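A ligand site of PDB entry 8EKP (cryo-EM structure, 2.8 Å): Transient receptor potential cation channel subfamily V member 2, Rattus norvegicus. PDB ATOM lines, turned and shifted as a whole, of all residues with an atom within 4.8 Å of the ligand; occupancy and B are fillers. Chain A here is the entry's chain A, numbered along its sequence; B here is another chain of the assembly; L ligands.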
ATOM      1  N   MET A 468      -1.730 -25.330 -10.385  1.00  0.00           N
ATOM      2  CA  MET A 468      -0.897 -24.610 -11.336  1.00  0.00           C
ATOM      3  C   MET A 468      -1.137 -25.057 -12.774  1.00  0.00           C
ATOM      4  O   MET A 468      -0.557 -24.483 -13.702  1.00  0.00           O
ATOM      5  CB  MET A 468       0.583 -24.786 -10.977  1.00  0.00           C
ATOM      6  N   ASP A 469      -1.991 -26.061 -12.978  1.00  0.00           N
ATOM      7  CA  ASP A 469      -2.310 -26.555 -14.307  1.00  0.00           C
ATOM      8  C   ASP A 469      -3.803 -26.528 -14.626  1.00  0.00           C
ATOM      9  O   ASP A 469      -4.176 -26.816 -15.761  1.00  0.00           O
ATOM     10  CB  ASP A 469      -1.792 -27.998 -14.475  1.00  0.00           C
ATOM     11  CG  ASP A 469      -1.435 -28.323 -15.904  1.00  0.00           C
ATOM     12  OD1 ASP A 469      -1.372 -27.402 -16.741  1.00  0.00           O
ATOM     13  OD2 ASP A 469      -1.186 -29.521 -16.196  1.00  0.00           O
ATOM     14  N   SER A 470      -4.656 -26.177 -13.656  1.00  0.00           N
ATOM     15  CA  SER A 470      -6.102 -26.173 -13.884  1.00  0.00           C
ATOM     16  C   SER A 470      -6.814 -24.975 -13.268  1.00  0.00           C
ATOM     17  O   SER A 470      -8.024 -25.046 -13.040  1.00  0.00           O
ATOM     18  CB  SER A 470      -6.725 -27.464 -13.350  1.00  0.00           C
ATOM     19  OG  SER A 470      -6.508 -27.604 -11.957  1.00  0.00           O
ATOM     20  N   TYR A 471      -6.100 -23.885 -12.978  1.00  0.00           N
ATOM     21  CA  TYR A 471      -6.732 -22.738 -12.331  1.00  0.00           C
ATOM     22  C   TYR A 471      -7.650 -21.967 -13.273  1.00  0.00           C
ATOM     23  O   TYR A 471      -8.501 -21.197 -12.793  1.00  0.00           O
ATOM     24  CB  TYR A 471      -5.676 -21.812 -11.714  1.00  0.00           C
ATOM     25  CG  TYR A 471      -4.749 -21.111 -12.688  1.00  0.00           C
ATOM     26  CD1 TYR A 471      -5.087 -19.893 -13.278  1.00  0.00           C
ATOM     27  CD2 TYR A 471      -3.494 -21.640 -12.976  1.00  0.00           C
ATOM     28  CE1 TYR A 471      -4.228 -19.257 -14.145  1.00  0.00           C
ATOM     29  CE2 TYR A 471      -2.630 -21.012 -13.845  1.00  0.00           C
ATOM     30  CZ  TYR A 471      -3.000 -19.817 -14.429  1.00  0.00           C
ATOM     31  OH  TYR A 471      -2.136 -19.189 -15.298  1.00  0.00           O
ATOM     32  N   PHE A 472      -7.519 -22.145 -14.593  1.00  0.00           N
ATOM     33  CA  PHE A 472      -8.459 -21.527 -15.505  1.00  0.00           C
ATOM     34  C   PHE A 472      -9.842 -22.158 -15.409  1.00  0.00           C
ATOM     35  O   PHE A 472     -10.840 -21.499 -15.700  1.00  0.00           O
ATOM     36  CB  PHE A 472      -7.942 -21.588 -16.942  1.00  0.00           C
ATOM     37  CG  PHE A 472      -7.134 -20.382 -17.348  1.00  0.00           C
ATOM     38  CD1 PHE A 472      -7.730 -19.136 -17.435  1.00  0.00           C
ATOM     39  CD2 PHE A 472      -5.792 -20.502 -17.643  1.00  0.00           C
ATOM     40  CE1 PHE A 472      -7.005 -18.028 -17.794  1.00  0.00           C
ATOM     41  CE2 PHE A 472      -5.050 -19.391 -18.026  1.00  0.00           C
ATOM     42  CZ  PHE A 472      -5.660 -18.156 -18.100  1.00  0.00           C
ATOM     43  N   LEU A 475     -11.204 -20.244 -12.595  1.00  0.00           N
ATOM     44  CA  LEU A 475     -11.494 -18.866 -12.965  1.00  0.00           C
ATOM     45  C   LEU A 475     -12.682 -18.777 -13.918  1.00  0.00           C
ATOM     46  O   LEU A 475     -13.431 -17.795 -13.897  1.00  0.00           O
ATOM     47  CB  LEU A 475     -10.261 -18.213 -13.580  1.00  0.00           C
ATOM     48  CG  LEU A 475      -9.102 -17.922 -12.628  1.00  0.00           C
ATOM     49  CD1 LEU A 475      -8.023 -17.111 -13.335  1.00  0.00           C
ATOM     50  CD2 LEU A 475      -9.593 -17.192 -11.380  1.00  0.00           C
ATOM     51  N   LEU A 478     -15.652 -19.184 -11.484  1.00  0.00           N
ATOM     52  CA  LEU A 478     -15.918 -18.013 -10.654  1.00  0.00           C
ATOM     53  C   LEU A 478     -16.460 -16.859 -11.487  1.00  0.00           C
ATOM     54  O   LEU A 478     -17.295 -16.078 -11.010  1.00  0.00           O
ATOM     55  CB  LEU A 478     -14.652 -17.601  -9.908  1.00  0.00           C
ATOM     56  CG  LEU A 478     -14.747 -16.418  -8.933  1.00  0.00           C
ATOM     57  CD1 LEU A 478     -15.716 -16.741  -7.794  1.00  0.00           C
ATOM     58  CD2 LEU A 478     -13.384 -16.050  -8.396  1.00  0.00           C
ATOM     59  N   LEU A 507     -12.580 -10.508 -14.811  1.00  0.00           N
ATOM     60  CA  LEU A 507     -12.229 -11.923 -14.744  1.00  0.00           C
ATOM     61  C   LEU A 507     -12.428 -12.629 -16.077  1.00  0.00           C
ATOM     62  O   LEU A 507     -11.707 -13.573 -16.399  1.00  0.00           O
ATOM     63  CB  LEU A 507     -13.044 -12.608 -13.653  1.00  0.00           C
ATOM     64  CG  LEU A 507     -12.407 -13.826 -12.988  1.00  0.00           C
ATOM     65  CD1 LEU A 507     -11.077 -13.450 -12.351  1.00  0.00           C
ATOM     66  CD2 LEU A 507     -13.339 -14.432 -11.959  1.00  0.00           C
ATOM     67  N   LEU A 510      -9.440 -11.539 -18.411  1.00  0.00           N
ATOM     68  CA  LEU A 510      -8.254 -12.291 -18.003  1.00  0.00           C
ATOM     69  C   LEU A 510      -8.343 -13.769 -18.360  1.00  0.00           C
ATOM     70  O   LEU A 510      -7.328 -14.463 -18.341  1.00  0.00           O
ATOM     71  CB  LEU A 510      -8.026 -12.143 -16.490  1.00  0.00           C
ATOM     72  CG  LEU A 510      -7.787 -10.735 -15.945  1.00  0.00           C
ATOM     73  CD1 LEU A 510      -7.707 -10.746 -14.423  1.00  0.00           C
ATOM     74  CD2 LEU A 510      -6.547 -10.104 -16.541  1.00  0.00           C
ATOM     75  N   LEU A 513      -6.578 -15.539 -21.838  1.00  0.00           N
ATOM     76  CA  LEU A 513      -5.215 -16.043 -21.884  1.00  0.00           C
ATOM     77  C   LEU A 513      -5.147 -17.568 -21.827  1.00  0.00           C
ATOM     78  O   LEU A 513      -4.068 -18.126 -22.055  1.00  0.00           O
ATOM     79  CB  LEU A 513      -4.414 -15.442 -20.736  1.00  0.00           C
ATOM     80  CG  LEU A 513      -4.420 -13.921 -20.747  1.00  0.00           C
ATOM     81  CD1 LEU A 513      -3.557 -13.419 -19.626  1.00  0.00           C
ATOM     82  CD2 LEU A 513      -3.938 -13.361 -22.073  1.00  0.00           C
ATOM     83  N   TYR A 514      -6.260 -18.241 -21.528  1.00  0.00           N
ATOM     84  CA  TYR A 514      -6.308 -19.688 -21.647  1.00  0.00           C
ATOM     85  C   TYR A 514      -6.156 -20.118 -23.103  1.00  0.00           C
ATOM     86  O   TYR A 514      -5.587 -21.183 -23.373  1.00  0.00           O
ATOM     87  CB  TYR A 514      -7.627 -20.210 -21.069  1.00  0.00           C
ATOM     88  CG  TYR A 514      -8.007 -21.611 -21.499  1.00  0.00           C
ATOM     89  CD1 TYR A 514      -7.438 -22.730 -20.888  1.00  0.00           C
ATOM     90  CD2 TYR A 514      -8.936 -21.825 -22.512  1.00  0.00           C
ATOM     91  CE1 TYR A 514      -7.776 -24.002 -21.282  1.00  0.00           C
ATOM     92  CE2 TYR A 514      -9.282 -23.102 -22.905  1.00  0.00           C
ATOM     93  CZ  TYR A 514      -8.699 -24.188 -22.296  1.00  0.00           C
ATOM     94  OH  TYR A 514      -9.043 -25.466 -22.679  1.00  0.00           O
ATOM     95  N   ARG A 517      -2.683 -20.970 -25.645  1.00  0.00           N
ATOM     96  CA  ARG A 517      -2.061 -22.267 -25.842  1.00  0.00           C
ATOM     97  C   ARG A 517      -2.401 -22.895 -27.181  1.00  0.00           C
ATOM     98  O   ARG A 517      -1.786 -23.913 -27.542  1.00  0.00           O
ATOM     99  CB  ARG A 517      -2.465 -23.212 -24.711  1.00  0.00           C
ATOM    100  CG  ARG A 517      -3.891 -23.714 -24.807  1.00  0.00           C
ATOM    101  CD  ARG A 517      -4.323 -24.370 -23.505  1.00  0.00           C
ATOM    102  NE  ARG A 517      -4.235 -23.444 -22.386  1.00  0.00           N
ATOM    103  CZ  ARG A 517      -4.174 -23.807 -21.117  1.00  0.00           C
ATOM    104  NH1 ARG A 517      -4.196 -25.073 -20.753  1.00  0.00           N
ATOM    105  NH2 ARG A 517      -4.097 -22.867 -20.180  1.00  0.00           N
ATOM    106  N   SER A 526       3.464 -18.309 -22.571  1.00  0.00           N
ATOM    107  CA  SER A 526       2.639 -18.414 -21.386  1.00  0.00           C
ATOM    108  C   SER A 526       3.147 -19.459 -20.409  1.00  0.00           C
ATOM    109  O   SER A 526       2.651 -19.507 -19.288  1.00  0.00           O
ATOM    110  CB  SER A 526       1.185 -18.727 -21.757  1.00  0.00           C
ATOM    111  OG  SER A 526       0.619 -17.668 -22.494  1.00  0.00           O
ATOM    112  N   VAL A 527       4.112 -20.293 -20.794  1.00  0.00           N
ATOM    113  CA  VAL A 527       4.736 -21.238 -19.881  1.00  0.00           C
ATOM    114  C   VAL A 527       6.011 -20.665 -19.266  1.00  0.00           C
ATOM    115  O   VAL A 527       6.247 -20.840 -18.073  1.00  0.00           O
ATOM    116  CB  VAL A 527       4.994 -22.580 -20.602  1.00  0.00           C
ATOM    117  CG1 VAL A 527       5.739 -23.542 -19.697  1.00  0.00           C
ATOM    118  CG2 VAL A 527       3.677 -23.194 -21.024  1.00  0.00           C
ATOM    119  N   ILE A 529       6.638 -17.665 -18.502  1.00  0.00           N
ATOM    120  CA  ILE A 529       6.383 -16.595 -17.544  1.00  0.00           C
ATOM    121  C   ILE A 529       6.080 -17.145 -16.157  1.00  0.00           C
ATOM    122  O   ILE A 529       6.566 -16.601 -15.163  1.00  0.00           O
ATOM    123  CB  ILE A 529       5.271 -15.643 -18.056  1.00  0.00           C
ATOM    124  CG1 ILE A 529       4.055 -16.407 -18.548  1.00  0.00           C
ATOM    125  CG2 ILE A 529       5.827 -14.727 -19.151  1.00  0.00           C
ATOM    126  CD1 ILE A 529       2.999 -15.496 -19.166  1.00  0.00           C
ATOM    127  N   GLN A 530       5.320 -18.242 -16.046  1.00  0.00           N
ATOM    128  CA  GLN A 530       5.183 -18.877 -14.731  1.00  0.00           C
ATOM    129  C   GLN A 530       6.412 -19.694 -14.335  1.00  0.00           C
ATOM    130  O   GLN A 530       6.315 -20.890 -14.095  1.00  0.00           O
ATOM    131  CB  GLN A 530       3.947 -19.766 -14.616  1.00  0.00           C
ATOM    132  CG  GLN A 530       2.562 -19.148 -14.417  1.00  0.00           C
ATOM    133  CD  GLN A 530       1.720 -19.057 -15.657  1.00  0.00           C
ATOM    134  OE1 GLN A 530       2.057 -19.604 -16.677  1.00  0.00           O
ATOM    135  NE2 GLN A 530       0.541 -18.502 -15.508  1.00  0.00           N
ATOM    136  N   LEU A 534       5.262 -17.607  -7.589  1.00  0.00           N
ATOM    137  CA  LEU A 534       4.060 -17.392  -6.788  1.00  0.00           C
ATOM    138  C   LEU A 534       4.268 -17.709  -5.316  1.00  0.00           C
ATOM    139  O   LEU A 534       3.893 -16.905  -4.453  1.00  0.00           O
ATOM    140  CB  LEU A 534       2.898 -18.203  -7.356  1.00  0.00           C
ATOM    141  CG  LEU A 534       2.204 -17.499  -8.517  1.00  0.00           C
ATOM    142  CD1 LEU A 534       1.456 -18.474  -9.413  1.00  0.00           C
ATOM    143  CD2 LEU A 534       1.281 -16.426  -7.969  1.00  0.00           C
ATOM    144  N   GLN A 663      -0.385 -29.034 -21.821  1.00  0.00           N
ATOM    145  CA  GLN A 663      -1.529 -28.141 -21.803  1.00  0.00           C
ATOM    146  C   GLN A 663      -2.493 -28.451 -22.945  1.00  0.00           C
ATOM    147  O   GLN A 663      -3.711 -28.370 -22.782  1.00  0.00           O
ATOM    148  CB  GLN A 663      -1.070 -26.682 -21.862  1.00  0.00           C
ATOM    149  CG  GLN A 663      -0.650 -26.113 -20.513  1.00  0.00           C
ATOM    150  CD  GLN A 663      -0.324 -24.643 -20.582  1.00  0.00           C
ATOM    151  OE1 GLN A 663      -0.300 -24.042 -21.657  1.00  0.00           O
ATOM    152  NE2 GLN A 663      -0.062 -24.046 -19.422  1.00  0.00           N
ATOM    153  N   VAL B 543      -0.276 -10.122 -23.518  1.00  0.00           N
ATOM    154  CA  VAL B 543      -0.814 -10.347 -22.178  1.00  0.00           C
ATOM    155  C   VAL B 543      -1.008  -9.025 -21.452  1.00  0.00           C
ATOM    156  O   VAL B 543      -2.046  -8.793 -20.813  1.00  0.00           O
ATOM    157  CB  VAL B 543       0.102 -11.307 -21.395  1.00  0.00           C
ATOM    158  CG1 VAL B 543      -0.396 -11.481 -19.990  1.00  0.00           C
ATOM    159  CG2 VAL B 543       0.172 -12.655 -22.092  1.00  0.00           C
ATOM    160  N   PHE B 547      -4.508  -7.209 -19.972  1.00  0.00           N
ATOM    161  CA  PHE B 547      -4.626  -6.693 -18.602  1.00  0.00           C
ATOM    162  C   PHE B 547      -5.018  -5.219 -18.607  1.00  0.00           C
ATOM    163  O   PHE B 547      -5.889  -4.795 -17.835  1.00  0.00           O
ATOM    164  CB  PHE B 547      -3.310  -6.867 -17.846  1.00  0.00           C
ATOM    165  CG  PHE B 547      -3.102  -8.233 -17.241  1.00  0.00           C
ATOM    166  CD1 PHE B 547      -3.289  -9.388 -17.995  1.00  0.00           C
ATOM    167  CD2 PHE B 547      -2.722  -8.363 -15.916  1.00  0.00           C
ATOM    168  CE1 PHE B 547      -3.089 -10.630 -17.435  1.00  0.00           C
ATOM    169  CE2 PHE B 547      -2.530  -9.610 -15.354  1.00  0.00           C
ATOM    170  CZ  PHE B 547      -2.711 -10.737 -16.109  1.00  0.00           C
ATOM    171  N   LEU B 632      -0.854  -7.466 -10.178  1.00  0.00           N
ATOM    172  CA  LEU B 632      -0.779  -8.338 -11.344  1.00  0.00           C
ATOM    173  C   LEU B 632       0.280  -7.850 -12.334  1.00  0.00           C
ATOM    174  O   LEU B 632       1.012  -8.655 -12.911  1.00  0.00           O
ATOM    175  CB  LEU B 632      -2.139  -8.435 -12.027  1.00  0.00           C
ATOM    176  CG  LEU B 632      -3.194  -9.338 -11.390  1.00  0.00           C
ATOM    177  CD1 LEU B 632      -4.569  -9.020 -11.953  1.00  0.00           C
ATOM    178  CD2 LEU B 632      -2.862 -10.803 -11.577  1.00  0.00           C
ATOM    179  N   VAL B 635       3.892  -8.461 -10.781  1.00  0.00           N
ATOM    180  CA  VAL B 635       4.242  -9.870 -10.878  1.00  0.00           C
ATOM    181  C   VAL B 635       4.596 -10.231 -12.318  1.00  0.00           C
ATOM    182  O   VAL B 635       5.580 -10.916 -12.590  1.00  0.00           O
ATOM    183  CB  VAL B 635       3.089 -10.749 -10.330  1.00  0.00           C
ATOM    184  CG1 VAL B 635       3.252 -12.205 -10.765  1.00  0.00           C
ATOM    185  CG2 VAL B 635       3.023 -10.659  -8.822  1.00  0.00           C
ATOM    186  N   LEU B 636       3.802  -9.728 -13.267  1.00  0.00           N
ATOM    187  CA  LEU B 636       3.975 -10.082 -14.665  1.00  0.00           C
ATOM    188  C   LEU B 636       5.205  -9.407 -15.278  1.00  0.00           C
ATOM    189  O   LEU B 636       5.862  -9.978 -16.148  1.00  0.00           O
ATOM    190  CB  LEU B 636       2.689  -9.755 -15.423  1.00  0.00           C
ATOM    191  CG  LEU B 636       2.374 -10.093 -16.861  1.00  0.00           C
ATOM    192  CD1 LEU B 636       0.899 -10.203 -16.901  1.00  0.00           C
ATOM    193  CD2 LEU B 636       2.733  -8.935 -17.738  1.00  0.00           C
ATOM    194  N   ASN B 639       8.023 -11.544 -13.898  1.00  0.00           N
ATOM    195  CA  ASN B 639       8.144 -12.773 -14.665  1.00  0.00           C
ATOM    196  C   ASN B 639       8.908 -12.542 -15.965  1.00  0.00           C
ATOM    197  O   ASN B 639       9.662 -13.415 -16.426  1.00  0.00           O
ATOM    198  CB  ASN B 639       6.760 -13.344 -14.968  1.00  0.00           C
ATOM    199  CG  ASN B 639       6.095 -13.955 -13.744  1.00  0.00           C
ATOM    200  OD1 ASN B 639       6.439 -13.626 -12.612  1.00  0.00           O
ATOM    201  ND2 ASN B 639       5.157 -14.864 -13.977  1.00  0.00           N
HETATM  202  O1  LIG L   1      -0.020 -20.624 -19.350  1.00  0.00           O
HETATM  203  O2  LIG L   1      -2.472 -20.517 -19.567  1.00  0.00           O
HETATM  204  P1  LIG L   1      -1.310 -20.306 -18.629  1.00  0.00           P
HETATM  205  O3  LIG L   1      -1.304 -18.744 -18.096  1.00  0.00           O
HETATM  206  C1  LIG L   1      -1.413 -17.712 -19.033  1.00  0.00           C
HETATM  207  C2  LIG L   1      -1.359 -16.373 -18.304  1.00  0.00           C
HETATM  208  C3  LIG L   1      -2.282 -16.438 -17.094  1.00  0.00           C
HETATM  209  O4  LIG L   1      -2.976 -15.235 -16.965  1.00  0.00           O
HETATM  210  C4  LIG L   1      -3.261 -14.868 -15.644  1.00  0.00           C
HETATM  211  O5  LIG L   1      -2.538 -14.115 -15.069  1.00  0.00           O
HETATM  212  C5  LIG L   1      -4.492 -15.426 -14.944  1.00  0.00           C
HETATM  213  C6  LIG L   1      -5.330 -14.277 -14.383  1.00  0.00           C
HETATM  214  C7  LIG L   1      -5.058 -14.145 -12.891  1.00  0.00           C
HETATM  215  C8  LIG L   1      -6.187 -13.362 -12.222  1.00  0.00           C
HETATM  216  C9  LIG L   1      -6.231 -13.703 -10.734  1.00  0.00           C
HETATM  217  C10 LIG L   1      -7.516 -13.157 -10.119  1.00  0.00           C
HETATM  218  C11 LIG L   1      -7.832 -13.958  -8.859  1.00  0.00           C
HETATM  219  C12 LIG L   1      -9.210 -13.554  -8.330  1.00  0.00           C
HETATM  220  C13 LIG L   1      -9.690 -14.586  -7.317  1.00  0.00           C
HETATM  221  O6  LIG L   1      -0.040 -16.142 -17.904  1.00  0.00           O
HETATM  222  C14 LIG L   1       0.162 -14.976 -17.153  1.00  0.00           C
HETATM  223  O7  LIG L   1      -0.246 -13.929 -17.527  1.00  0.00           O
HETATM  224  C15 LIG L   1       0.942 -15.061 -15.837  1.00  0.00           C
HETATM  225  C16 LIG L   1       1.588 -13.720 -15.512  1.00  0.00           C
HETATM  226  C17 LIG L   1       0.788 -13.032 -14.410  1.00  0.00           C
HETATM  227  C18 LIG L   1       0.719 -13.933 -13.181  1.00  0.00           C
HETATM  228  C19 LIG L   1      -0.233 -13.317 -12.158  1.00  0.00           C
HETATM  229  C20 LIG L   1      -0.336 -14.204 -10.930  1.00  0.00           C
HETATM  230  C21 LIG L   1      -1.803 -14.331 -10.521  1.00  0.00           C
HETATM  231  C22 LIG L   1      -1.907 -14.508  -9.013  1.00  0.00           C
HETATM  232  C23 LIG L   1      -1.458 -13.232  -8.316  1.00  0.00           C
HETATM  233  O8  LIG L   1      -1.459 -21.320 -17.333  1.00  0.00           O
HETATM  234  C24 LIG L   1      -2.590 -22.144 -17.261  1.00  0.00           C
HETATM  235  C25 LIG L   1      -2.204 -23.464 -16.603  1.00  0.00           C
HETATM  236  N1  LIG L   1      -1.078 -23.254 -15.718  1.00  0.00           N
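The side-chain amide nitrogen (NE2) of Gln 663 is in hydrogen-bond range of an oxygen (O1) of the ligand. The backbone carbonyl oxygen (O) of Met 468 is in hydrogen-bond range of a nitrogen (N1) of the ligand (2.4 Å). NH2 of Arg 517 is in salt-bridge range of O2 of the ligand, at 2.9 Å. O3 of the ligand lies within hydrogen-bond range of NE2 of Gln 530, at 3.2 Å. An oxygen (O3) of the ligand is in hydrogen-bond range of the side-chain hydroxyl of Tyr 471 (3.0 Å). O of Ser 526 sits close to O1 of the ligand, 2.9 Å away.
O of Ile 529 lies within hydrogen-bond range of ND2 of Asn 639 of chain B (2.5 Å). OH of Tyr 471 lies within hydrogen-bond range of NE2 of Gln 530 (2.8 Å). The backbone carbonyl oxygen (O) of Val 635 of chain B sits close to the side-chain amide oxygen (OD1) of Asn 639 of chain B, at 2.8 Å. The guanidinium group (NE) of Arg 517 is in hydrogen-bond range of the backbone carbonyl oxygen (O) of Tyr 514 (2.8 Å). The side-chain amide oxygen of Gln 530 sits close to the backbone carbonyl oxygen of Ser 526.
Asp 469 touches the ligand. Phe 472 touches the ligand (CE2 to O2, 3.2 Å). CD1 of Leu 510 touches C8 of the ligand, 3.7 Å away. Leu 513 touches the ligand (CD1 to O4, 3.3 Å). Ile 529 touches the ligand. Leu 534 touches the ligand (CD2 to C22, 3.9 Å). CG1 of Val 543 of chain B touches O7 of the ligand, 3.5 Å away. Phe 547 of chain B touches the ligand. Leu 632 of chain B touches the ligand. Val 635 of chain B touches the ligand (CG1 to C18, 3.9 Å). Leu 636 of chain B touches the ligand (CD1 to C17, 3.8 Å). Hydrophobic or aromatic side chains within 4 Å of the ligand: Tyr 471, Phe 472, Leu 510, Leu 513, Ile 529, Leu 534, Val 543 of chain B, Phe 547 of chain B, Leu 632 of chain B, Val 635 of chain B and Leu 636 of chain B. 17 residues have an atom within 4 Å of the ligand: Met 468, Asp 469, Tyr 471, Phe 472, Leu 510, Leu 513, Arg 517, Ser 526, Ile 529, Gln 530, Leu 534, Gln 663, Val 543 of chain B, Phe 547 of chain B, Leu 632 of chain B, Val 635 of chain B and Leu 636 of chain B. Along chain A the residues within 4 Å of the ligand span positions 468 to 663.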
